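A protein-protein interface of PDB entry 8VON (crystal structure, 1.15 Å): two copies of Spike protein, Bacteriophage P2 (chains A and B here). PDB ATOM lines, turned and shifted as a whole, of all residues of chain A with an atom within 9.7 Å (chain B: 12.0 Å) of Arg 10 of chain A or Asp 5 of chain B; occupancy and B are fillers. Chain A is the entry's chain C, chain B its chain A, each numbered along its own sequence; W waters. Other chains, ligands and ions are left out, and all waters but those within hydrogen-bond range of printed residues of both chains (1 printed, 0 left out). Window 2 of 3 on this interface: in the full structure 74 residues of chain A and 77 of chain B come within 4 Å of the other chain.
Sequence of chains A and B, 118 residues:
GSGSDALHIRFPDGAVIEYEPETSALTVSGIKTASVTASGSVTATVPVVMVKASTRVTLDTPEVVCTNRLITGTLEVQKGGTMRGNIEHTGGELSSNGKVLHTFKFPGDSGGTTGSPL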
ATOM      1  N   LEU A   7     -19.089 -28.725 -29.713  1.00  0.00           N
ATOM      2  CA  LEU A   7     -19.909 -27.975 -28.766  1.00  0.00           C
ATOM      3  C   LEU A   7     -20.980 -27.247 -29.574  1.00  0.00           C
ATOM      4  O   LEU A   7     -20.676 -26.307 -30.314  1.00  0.00           O
ATOM      5  CB  LEU A   7     -19.057 -26.990 -27.968  1.00  0.00           C
ATOM      6  CG  LEU A   7     -19.834 -26.088 -27.004  1.00  0.00           C
ATOM      7  CD1 LEU A   7     -20.532 -26.884 -25.916  1.00  0.00           C
ATOM      8  CD2 LEU A   7     -18.900 -25.072 -26.394  1.00  0.00           C
ATOM      9  N   HIS A   8     -22.230 -27.654 -29.396  1.00  0.00           N
ATOM     10  CA  HIS A   8     -23.324 -26.970 -30.058  1.00  0.00           C
ATOM     11  C   HIS A   8     -24.591 -27.287 -29.286  1.00  0.00           C
ATOM     12  O   HIS A   8     -25.102 -28.403 -29.362  1.00  0.00           O
ATOM     13  CB  HIS A   8     -23.466 -27.385 -31.483  1.00  0.00           C
ATOM     14  CG  HIS A   8     -24.614 -26.698 -32.130  1.00  0.00           C
ATOM     15  ND1 HIS A   8     -25.901 -27.178 -32.084  1.00  0.00           N
ATOM     16  CD2 HIS A   8     -24.700 -25.464 -32.676  1.00  0.00           C
ATOM     17  CE1 HIS A   8     -26.714 -26.331 -32.680  1.00  0.00           C
ATOM     18  NE2 HIS A   8     -26.014 -25.269 -33.032  1.00  0.00           N
ATOM     19  N   ILE A   9     -25.082 -26.324 -28.528  1.00  0.00           N
ATOM     20  CA  ILE A   9     -26.252 -26.519 -27.694  1.00  0.00           C
ATOM     21  C   ILE A   9     -27.280 -25.454 -28.036  1.00  0.00           C
ATOM     22  O   ILE A   9     -26.976 -24.265 -27.969  1.00  0.00           O
ATOM     23  CB  ILE A   9     -25.931 -26.435 -26.197  1.00  0.00           C
ATOM     24  CG1 ILE A   9     -24.681 -27.214 -25.831  1.00  0.00           C
ATOM     25  CG2 ILE A   9     -27.151 -26.906 -25.407  1.00  0.00           C
ATOM     26  CD1 ILE A   9     -24.231 -26.969 -24.397  1.00  0.00           C
ATOM     27  N   ARG A  10     -28.491 -25.880 -28.381  1.00  0.00           N
ATOM     28  CA  ARG A  10     -29.631 -24.996 -28.568  1.00  0.00           C
ATOM     29  C   ARG A  10     -30.604 -25.283 -27.434  1.00  0.00           C
ATOM     30  O   ARG A  10     -31.054 -26.422 -27.271  1.00  0.00           O
ATOM     31  CB  ARG A  10     -30.302 -25.231 -29.917  1.00  0.00           C
ATOM     32  CG  ARG A  10     -31.366 -24.193 -30.266  1.00  0.00           C
ATOM     33  CD  ARG A  10     -32.762 -24.556 -29.805  1.00  0.00           C
ATOM     34  NE  ARG A  10     -33.670 -23.424 -29.947  1.00  0.00           N
ATOM     35  CZ  ARG A  10     -34.955 -23.442 -29.618  1.00  0.00           C
ATOM     36  NH1 ARG A  10     -35.495 -24.481 -29.003  1.00  0.00           N
ATOM     37  NH2 ARG A  10     -35.719 -22.396 -29.928  1.00  0.00           N
ATOM     38  N   PHE A  11     -30.900 -24.286 -26.655  1.00  0.00           N
ATOM     39  CA  PHE A  11     -31.737 -24.437 -25.481  1.00  0.00           C
ATOM     40  C   PHE A  11     -33.173 -24.074 -25.806  1.00  0.00           C
ATOM     41  O   PHE A  11     -33.454 -23.391 -26.796  1.00  0.00           O
ATOM     42  CB  PHE A  11     -31.203 -23.513 -24.393  1.00  0.00           C
ATOM     43  CG  PHE A  11     -29.849 -23.895 -23.882  1.00  0.00           C
ATOM     44  CD1 PHE A  11     -29.705 -24.864 -22.901  1.00  0.00           C
ATOM     45  CD2 PHE A  11     -28.705 -23.300 -24.391  1.00  0.00           C
ATOM     46  CE1 PHE A  11     -28.461 -25.188 -22.418  1.00  0.00           C
ATOM     47  CE2 PHE A  11     -27.446 -23.641 -23.901  1.00  0.00           C
ATOM     48  CZ  PHE A  11     -27.338 -24.580 -22.908  1.00  0.00           C
ATOM     49  N   PRO A  12     -34.119 -24.473 -24.958  1.00  0.00           N
ATOM     50  CA  PRO A  12     -35.537 -24.246 -25.291  1.00  0.00           C
ATOM     51  C   PRO A  12     -35.984 -22.801 -25.243  1.00  0.00           C
ATOM     52  O   PRO A  12     -37.077 -22.502 -25.752  1.00  0.00           O
ATOM     53  CB  PRO A  12     -36.293 -25.119 -24.284  1.00  0.00           C
ATOM     54  CG  PRO A  12     -35.318 -25.411 -23.191  1.00  0.00           C
ATOM     55  CD  PRO A  12     -33.941 -25.352 -23.789  1.00  0.00           C
ATOM     56  N   ASP A  13     -35.198 -21.908 -24.657  1.00  0.00           N
ATOM     57  CA  ASP A  13     -35.463 -20.486 -24.710  1.00  0.00           C
ATOM     58  C   ASP A  13     -34.926 -19.831 -25.975  1.00  0.00           C
ATOM     59  O   ASP A  13     -35.054 -18.612 -26.109  1.00  0.00           O
ATOM     60  CB  ASP A  13     -34.888 -19.797 -23.467  1.00  0.00           C
ATOM     61  CG  ASP A  13     -33.387 -19.898 -23.375  1.00  0.00           C
ATOM     62  OD1 ASP A  13     -32.783 -20.707 -24.117  1.00  0.00           O
ATOM     63  OD2 ASP A  13     -32.815 -19.148 -22.553  1.00  0.00           O
ATOM     64  N   GLY A  14     -34.333 -20.590 -26.899  1.00  0.00           N
ATOM     65  CA  GLY A  14     -33.727 -20.035 -28.088  1.00  0.00           C
ATOM     66  C   GLY A  14     -32.269 -19.680 -27.945  1.00  0.00           C
ATOM     67  O   GLY A  14     -31.641 -19.304 -28.952  1.00  0.00           O
ATOM     68  N   ALA A  15     -31.691 -19.819 -26.765  1.00  0.00           N
ATOM     69  CA  ALA A  15     -30.276 -19.521 -26.618  1.00  0.00           C
ATOM     70  C   ALA A  15     -29.429 -20.565 -27.321  1.00  0.00           C
ATOM     71  O   ALA A  15     -29.811 -21.725 -27.474  1.00  0.00           O
ATOM     72  CB  ALA A  15     -29.894 -19.465 -25.150  1.00  0.00           C
ATOM     73  N   VAL A  16     -28.235 -20.140 -27.710  1.00  0.00           N
ATOM     74  CA  VAL A  16     -27.238 -21.015 -28.305  1.00  0.00           C
ATOM     75  C   VAL A  16     -25.918 -20.812 -27.600  1.00  0.00           C
ATOM     76  O   VAL A  16     -25.503 -19.677 -27.373  1.00  0.00           O
ATOM     77  CB  VAL A  16     -27.064 -20.749 -29.812  1.00  0.00           C
ATOM     78  CG1 VAL A  16     -25.913 -21.579 -30.378  1.00  0.00           C
ATOM     79  CG2 VAL A  16     -28.354 -21.038 -30.546  1.00  0.00           C
ATOM     80  N   ILE A  17     -25.261 -21.911 -27.284  1.00  0.00           N
ATOM     81  CA  ILE A  17     -23.866 -21.925 -26.873  1.00  0.00           C
ATOM     82  C   ILE A  17     -23.184 -22.885 -27.828  1.00  0.00           C
ATOM     83  O   ILE A  17     -23.532 -24.066 -27.877  1.00  0.00           O
ATOM     84  CB  ILE A  17     -23.700 -22.370 -25.410  1.00  0.00           C
ATOM     85  CG1 ILE A  17     -24.352 -21.358 -24.460  1.00  0.00           C
ATOM     86  CG2 ILE A  17     -22.207 -22.541 -25.076  1.00  0.00           C
ATOM     87  CD1 ILE A  17     -24.369 -21.755 -22.978  1.00  0.00           C
ATOM     88  N   GLU A  18     -22.207 -22.389 -28.573  1.00  0.00           N
ATOM     89  CA  GLU A  18     -21.569 -23.231 -29.563  1.00  0.00           C
ATOM     90  C   GLU A  18     -20.153 -22.779 -29.835  1.00  0.00           C
ATOM     91  O   GLU A  18     -19.789 -21.624 -29.621  1.00  0.00           O
ATOM     92  CB  GLU A  18     -22.365 -23.238 -30.873  1.00  0.00           C
ATOM     93  CG  GLU A  18     -22.245 -21.947 -31.623  1.00  0.00           C
ATOM     94  CD  GLU A  18     -22.792 -21.994 -33.018  1.00  0.00           C
ATOM     95  OE1 GLU A  18     -22.332 -21.203 -33.850  1.00  0.00           O
ATOM     96  OE2 GLU A  18     -23.656 -22.825 -33.302  1.00  0.00           O
ATOM     97  N   TYR A  19     -19.378 -23.717 -30.358  1.00  0.00           N
ATOM     98  CA  TYR A  19     -18.105 -23.412 -30.980  1.00  0.00           C
ATOM     99  C   TYR A  19     -18.170 -23.898 -32.422  1.00  0.00           C
ATOM    100  O   TYR A  19     -18.531 -25.048 -32.673  1.00  0.00           O
ATOM    101  CB  TYR A  19     -16.933 -24.065 -30.277  1.00  0.00           C
ATOM    102  CG  TYR A  19     -15.621 -23.588 -30.857  1.00  0.00           C
ATOM    103  CD1 TYR A  19     -15.211 -22.287 -30.665  1.00  0.00           C
ATOM    104  CD2 TYR A  19     -14.843 -24.400 -31.648  1.00  0.00           C
ATOM    105  CE1 TYR A  19     -14.060 -21.819 -31.216  1.00  0.00           C
ATOM    106  CE2 TYR A  19     -13.649 -23.929 -32.202  1.00  0.00           C
ATOM    107  CZ  TYR A  19     -13.278 -22.636 -31.976  1.00  0.00           C
ATOM    108  OH  TYR A  19     -12.108 -22.121 -32.480  1.00  0.00           O
ATOM    109  N   THR A  27     -19.527 -18.756 -29.649  1.00  0.00           N
ATOM    110  CA  THR A  27     -20.692 -17.890 -29.620  1.00  0.00           C
ATOM    111  C   THR A  27     -21.644 -18.288 -28.512  1.00  0.00           C
ATOM    112  O   THR A  27     -22.013 -19.457 -28.391  1.00  0.00           O
ATOM    113  CB  THR A  27     -21.441 -17.973 -30.961  1.00  0.00           C
ATOM    114  OG1 THR A  27     -20.537 -17.596 -32.008  1.00  0.00           O
ATOM    115  CG2 THR A  27     -22.682 -17.108 -30.992  1.00  0.00           C
ATOM    116  N   SER A  29     -25.419 -16.742 -27.561  1.00  0.00           N
ATOM    117  CA  SER A  29     -26.414 -15.782 -28.013  1.00  0.00           C
ATOM    118  C   SER A  29     -27.783 -16.151 -27.471  1.00  0.00           C
ATOM    119  O   SER A  29     -28.025 -17.282 -27.054  1.00  0.00           O
ATOM    120  CB  SER A  29     -26.470 -15.700 -29.536  1.00  0.00           C
ATOM    121  OG  SER A  29     -26.906 -16.933 -30.056  1.00  0.00           O
ATOM    122  N   GLY A  30     -28.687 -15.176 -27.518  1.00  0.00           N
ATOM    123  CA  GLY A  30     -30.062 -15.426 -27.156  1.00  0.00           C
ATOM    124  C   GLY A  30     -30.283 -15.579 -25.672  1.00  0.00           C
ATOM    125  O   GLY A  30     -31.329 -16.086 -25.263  1.00  0.00           O
ATOM    126  N   ASP B   5     -29.497 -30.365 -25.294  1.00  0.00           N
ATOM    127  CA  ASP B   5     -30.062 -29.037 -25.084  1.00  0.00           C
ATOM    128  C   ASP B   5     -30.034 -28.583 -23.623  1.00  0.00           C
ATOM    129  O   ASP B   5     -30.917 -27.847 -23.179  1.00  0.00           O
ATOM    130  CB  ASP B   5     -31.512 -28.989 -25.589  1.00  0.00           C
ATOM    131  CG  ASP B   5     -32.431 -29.918 -24.812  1.00  0.00           C
ATOM    132  OD1 ASP B   5     -31.919 -30.751 -24.029  1.00  0.00           O
ATOM    133  OD2 ASP B   5     -33.666 -29.810 -24.983  1.00  0.00           O
ATOM    134  N   ALA B   6     -29.009 -28.998 -22.884  1.00  0.00           N
ATOM    135  CA  ALA B   6     -28.868 -28.615 -21.483  1.00  0.00           C
ATOM    136  C   ALA B   6     -27.393 -28.487 -21.141  1.00  0.00           C
ATOM    137  O   ALA B   6     -26.536 -29.004 -21.868  1.00  0.00           O
ATOM    138  CB  ALA B   6     -29.528 -29.647 -20.561  1.00  0.00           C
ATOM    139  N   LEU B   7     -27.124 -27.799 -20.011  1.00  0.00           N
ATOM    140  CA  LEU B   7     -25.775 -27.502 -19.520  1.00  0.00           C
ATOM    141  C   LEU B   7     -25.776 -27.281 -17.994  1.00  0.00           C
ATOM    142  O   LEU B   7     -26.227 -26.239 -17.504  1.00  0.00           O
ATOM    143  CB  LEU B   7     -25.204 -26.309 -20.285  1.00  0.00           C
ATOM    144  CG  LEU B   7     -23.802 -25.834 -19.897  1.00  0.00           C
ATOM    145  CD1 LEU B   7     -22.761 -26.913 -20.067  1.00  0.00           C
ATOM    146  CD2 LEU B   7     -23.420 -24.534 -20.621  1.00  0.00           C
ATOM    147  N   HIS B   8     -25.269 -28.273 -17.250  1.00  0.00           N
ATOM    148  CA  HIS B   8     -25.096 -28.218 -15.791  1.00  0.00           C
ATOM    149  C   HIS B   8     -23.837 -29.046 -15.516  1.00  0.00           C
ATOM    150  O   HIS B   8     -23.910 -30.265 -15.576  1.00  0.00           O
ATOM    151  CB  HIS B   8     -26.291 -28.936 -15.170  1.00  0.00           C
ATOM    152  CG  HIS B   8     -27.103 -28.132 -14.206  1.00  0.00           C
ATOM    153  ND1 HIS B   8     -28.477 -28.064 -14.293  1.00  0.00           N
ATOM    154  CD2 HIS B   8     -26.760 -27.413 -13.113  1.00  0.00           C
ATOM    155  CE1 HIS B   8     -28.943 -27.303 -13.319  1.00  0.00           C
ATOM    156  NE2 HIS B   8     -27.920 -26.901 -12.585  1.00  0.00           N
ATOM    157  N   ILE B   9     -22.705 -28.415 -15.259  1.00  0.00           N
ATOM    158  CA  ILE B   9     -21.443 -29.096 -15.002  1.00  0.00           C
ATOM    159  C   ILE B   9     -20.978 -28.703 -13.610  1.00  0.00           C
ATOM    160  O   ILE B   9     -20.931 -27.512 -13.292  1.00  0.00           O
ATOM    161  CB  ILE B   9     -20.380 -28.678 -16.034  1.00  0.00           C
ATOM    162  CG1 ILE B   9     -20.906 -28.814 -17.452  1.00  0.00           C
ATOM    163  CG2 ILE B   9     -19.087 -29.479 -15.832  1.00  0.00           C
ATOM    164  CD1 ILE B   9     -19.934 -28.306 -18.478  1.00  0.00           C
ATOM    165  N   ILE B  17     -20.348 -24.685 -14.229  1.00  0.00           N
ATOM    166  CA  ILE B  17     -20.728 -24.027 -15.472  1.00  0.00           C
ATOM    167  C   ILE B  17     -22.151 -24.468 -15.779  1.00  0.00           C
ATOM    168  O   ILE B  17     -22.402 -25.670 -15.884  1.00  0.00           O
ATOM    169  CB  ILE B  17     -19.770 -24.397 -16.617  1.00  0.00           C
ATOM    170  CG1 ILE B  17     -18.343 -23.921 -16.324  1.00  0.00           C
ATOM    171  CG2 ILE B  17     -20.280 -23.811 -17.928  1.00  0.00           C
ATOM    172  CD1 ILE B  17     -17.298 -24.467 -17.287  1.00  0.00           C
ATOM    173  N   GLU B  18     -23.074 -23.510 -15.893  1.00  0.00           N
ATOM    174  CA  GLU B  18     -24.457 -23.882 -16.047  1.00  0.00           C
ATOM    175  C   GLU B  18     -25.188 -22.865 -16.908  1.00  0.00           C
ATOM    176  O   GLU B  18     -24.854 -21.680 -16.939  1.00  0.00           O
ATOM    177  CB  GLU B  18     -25.192 -23.977 -14.717  1.00  0.00           C
ATOM    178  CG  GLU B  18     -25.245 -22.707 -13.977  1.00  0.00           C
ATOM    179  CD  GLU B  18     -26.354 -22.660 -12.921  1.00  0.00           C
ATOM    180  OE1 GLU B  18     -27.575 -22.353 -13.334  1.00  0.00           O
ATOM    181  OE2 GLU B  18     -25.971 -22.928 -11.737  1.00  0.00           O
ATOM    182  N   TYR B  19     -26.208 -23.349 -17.597  1.00  0.00           N
ATOM    183  CA  TYR B  19     -27.124 -22.481 -18.319  1.00  0.00           C
ATOM    184  C   TYR B  19     -28.538 -22.825 -17.877  1.00  0.00           C
ATOM    185  O   TYR B  19     -28.943 -23.992 -17.938  1.00  0.00           O
ATOM    186  CB  TYR B  19     -27.013 -22.576 -19.849  1.00  0.00           C
ATOM    187  CG  TYR B  19     -27.884 -21.532 -20.488  1.00  0.00           C
ATOM    188  CD1 TYR B  19     -27.529 -20.198 -20.437  1.00  0.00           C
ATOM    189  CD2 TYR B  19     -29.101 -21.862 -21.077  1.00  0.00           C
ATOM    190  CE1 TYR B  19     -28.332 -19.225 -20.956  1.00  0.00           C
ATOM    191  CE2 TYR B  19     -29.918 -20.878 -21.612  1.00  0.00           C
ATOM    192  CZ  TYR B  19     -29.521 -19.561 -21.536  1.00  0.00           C
ATOM    193  OH  TYR B  19     -30.293 -18.561 -22.064  1.00  0.00           O
ATOM    194  N   GLU B  20     -29.284 -21.812 -17.465  1.00  0.00           N
ATOM    195  CA  GLU B  20     -30.645 -21.961 -16.962  1.00  0.00           C
ATOM    196  C   GLU B  20     -31.617 -21.333 -17.951  1.00  0.00           C
ATOM    197  O   GLU B  20     -31.732 -20.105 -17.995  1.00  0.00           O
ATOM    198  CB  GLU B  20     -30.762 -21.278 -15.604  1.00  0.00           C
ATOM    199  CG  GLU B  20     -32.144 -21.351 -15.024  1.00  0.00           C
ATOM    200  CD  GLU B  20     -32.702 -22.744 -15.075  1.00  0.00           C
ATOM    201  OE1 GLU B  20     -32.194 -23.613 -14.332  1.00  0.00           O
ATOM    202  OE2 GLU B  20     -33.621 -22.976 -15.890  1.00  0.00           O
ATOM    203  N   PRO B  21     -32.332 -22.126 -18.758  1.00  0.00           N
ATOM    204  CA  PRO B  21     -33.247 -21.530 -19.746  1.00  0.00           C
ATOM    205  C   PRO B  21     -34.429 -20.808 -19.132  1.00  0.00           C
ATOM    206  O   PRO B  21     -35.005 -19.952 -19.795  1.00  0.00           O
ATOM    207  CB  PRO B  21     -33.676 -22.727 -20.610  1.00  0.00           C
ATOM    208  CG  PRO B  21     -32.690 -23.770 -20.354  1.00  0.00           C
ATOM    209  CD  PRO B  21     -32.223 -23.573 -18.930  1.00  0.00           C
ATOM    210  N   GLU B  22     -34.832 -21.111 -17.895  1.00  0.00           N
ATOM    211  CA  GLU B  22     -36.026 -20.470 -17.343  1.00  0.00           C
ATOM    212  C   GLU B  22     -35.830 -18.970 -17.186  1.00  0.00           C
ATOM    213  O   GLU B  22     -36.789 -18.202 -17.349  1.00  0.00           O
ATOM    214  CB  GLU B  22     -36.344 -21.080 -15.985  1.00  0.00           C
ATOM    215  CG  GLU B  22     -37.024 -22.419 -16.061  1.00  0.00           C
ATOM    216  CD  GLU B  22     -38.419 -22.313 -16.620  1.00  0.00           C
ATOM    217  OE1 GLU B  22     -38.591 -22.503 -17.835  1.00  0.00           O
ATOM    218  OE2 GLU B  22     -39.341 -21.970 -15.874  1.00  0.00           O
ATOM    219  N   THR B  23     -34.619 -18.548 -16.821  1.00  0.00           N
ATOM    220  CA  THR B  23     -34.252 -17.153 -16.669  1.00  0.00           C
ATOM    221  C   THR B  23     -33.230 -16.747 -17.722  1.00  0.00           C
ATOM    222  O   THR B  23     -32.737 -15.620 -17.697  1.00  0.00           O
ATOM    223  CB  THR B  23     -33.676 -16.940 -15.266  1.00  0.00           C
ATOM    224  OG1 THR B  23     -32.603 -17.872 -15.143  1.00  0.00           O
ATOM    225  CG2 THR B  23     -34.717 -17.180 -14.180  1.00  0.00           C
ATOM    226  N   SER B  24     -32.930 -17.628 -18.653  1.00  0.00           N
ATOM    227  CA  SER B  24     -31.930 -17.404 -19.693  1.00  0.00           C
ATOM    228  C   SER B  24     -30.610 -16.895 -19.126  1.00  0.00           C
ATOM    229  O   SER B  24     -30.051 -15.890 -19.592  1.00  0.00           O
ATOM    230  CB  SER B  24     -32.469 -16.480 -20.771  1.00  0.00           C
ATOM    231  OG  SER B  24     -33.671 -16.980 -21.357  1.00  0.00           O
ATOM    232  N   ALA B  25     -30.098 -17.607 -18.122  1.00  0.00           N
ATOM    233  CA  ALA B  25     -28.932 -17.175 -17.351  1.00  0.00           C
ATOM    234  C   ALA B  25     -27.778 -18.156 -17.473  1.00  0.00           C
ATOM    235  O   ALA B  25     -27.914 -19.333 -17.130  1.00  0.00           O
ATOM    236  CB  ALA B  25     -29.318 -17.051 -15.879  1.00  0.00           C
ATOM    237  N   LEU B  26     -26.642 -17.656 -17.954  1.00  0.00           N
ATOM    238  CA  LEU B  26     -25.394 -18.401 -18.003  1.00  0.00           C
ATOM    239  C   LEU B  26     -24.568 -18.064 -16.766  1.00  0.00           C
ATOM    240  O   LEU B  26     -24.357 -16.886 -16.474  1.00  0.00           O
ATOM    241  CB  LEU B  26     -24.625 -18.003 -19.267  1.00  0.00           C
ATOM    242  CG  LEU B  26     -23.230 -18.607 -19.428  1.00  0.00           C
ATOM    243  CD1 LEU B  26     -23.286 -20.105 -19.520  1.00  0.00           C
ATOM    244  CD2 LEU B  26     -22.556 -18.015 -20.657  1.00  0.00           C
HETATM  245  O   HOH W   1     -33.535 -15.235 -23.675  1.00  0.00           O
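OH of Tyr 19 of chain B is in hydrogen-bond range of OD2 of Asp 13 of chain A.
The side-chain carboxylate of Asp 13 of chain A lies within hydrogen-bond range of the side-chain hydroxyl of Ser 24 of chain B, 2.6 Å away.
The backbone carbonyl oxygen of Leu 7 of chain B sits at hydrogen-bond distance from the backbone NH of Tyr 19 of chain B, 2.9 Å away.
The backbone NH (N) of Ile 9 of chain A is in hydrogen-bond range of the backbone carbonyl oxygen (O) of Ile 17 of chain A.
OD1 of Asp 13 of chain A lies within hydrogen-bond range of N of Ala 15 of chain A, at 3.0 Å.
Ile 9 of chain A touches Asp 5 of chain B (CG2 to CA, 3.6 Å).
Ala 6 of chain B touches Ile 9 of chain A (N to CG2, 3.8 Å).
Arg 10 of chain A touches Asp 5 of chain B (O to CB, 3.1 Å).
CD1 of Phe 11 of chain A touches O of Asp 5 of chain B, 3.2 Å away.
CE1 of Phe 11 of chain A touches N of Leu 7 of chain B, 3.8 Å away.
Phe 11 of chain A touches Tyr 19 of chain B (CG to CD2, 3.5 Å).
CD of Pro 12 of chain A touches O of Asp 5 of chain B (3.97 Å).
Ala 15 of chain A touches Tyr 19 of chain B (CB to OH, 3.2 Å).
Leu 7 of chain B touches Ile 17 of chain A (CD2 to CD1, 3.8 Å).
CD1 of Ile 17 of chain A touches CD1 of Leu 26 of chain B, at 3.98 Å.
Of the printed residues of chain B, Arg 10 of chain A touches Asp 5 (3.1 Å).
Printed residues of chain A within 4 Å of Asp 5 of chain B: Ile 9, Arg 10, Phe 11 and Pro 12.
No residue of chain B comes within 4 Å of His 8 of chain A.
Of chain B, only Asp 5 and Ala 6 come within 4 Å of Ile 9 of chain A.
Phe 11 of chain A touches just these residues of chain B: Asp 5, Ala 6, Leu 7 and Tyr 19.
No residue of chain B comes within 4 Å of Gly 14 of chain A.
Ala 6 of chain B touches just these residues of chain A: Ile 9 (3.8 Å) and Phe 11 (3.6 Å).
Of the printed residues of chain B, Ile 17 of chain A touches Leu 7 and Leu 26.
Of the printed residues of chain A, Ser 24 of chain B touches Asp 13 (2.6 Å).
Printed residues of chain B within 4 Å of Asp 13 of chain A: Tyr 19, Pro 21 and Ser 24.
Of the printed residues of chain A, Leu 7 of chain B touches Phe 11 (3.8 Å) and Ile 17 (3.8 Å).
Printed residues of chain A within 4 Å of Pro 21 of chain B: Pro 12 (3.98 Å) and Asp 13 (3.6 Å).
The nearest printed residue of chain B that does not touch Arg 10 of chain A is Ala 6 of chain B (5.5 Å).
The nearest printed residue of chain A that does not touch Asp 5 of chain B is His 8 of chain A (6.3 Å).
Of the 16 printed residues of chain A, 7 touch a printed residue of chain B.
Hydrophobic or aromatic side chains of chain A within 4 Å of the printed part of chain B: Ile 9, Phe 11, Pro 12, Ala 15 and Ile 17.
Printed residues of chain B that touch a printed residue of chain A: Asp 5, Ala 6, Leu 7, Tyr 19, Pro 21, Ser 24 and Leu 26.
Along chain B the printed residues that touch a printed residue of chain A span positions 5 to 26.
Among the printed residues, 15 pairs touch across the chains.
Among the printed residues, no Asp or Glu carboxylate lies within 4 Å of a Lys or Arg side-chain nitrogen of the other chain.
Ile 17 of chain A touches Leu 7 of chain B, but with the chains exchanged Leu 7 of chain A does not touch Ile 17 of chain B (8.6 Å).
Water W1 lies within hydrogen-bond range of the backbone carbonyl oxygen of Gly 30 of chain A (2.8 Å) and the side-chain hydroxyl of Ser 24 of chain B (2.9 Å).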
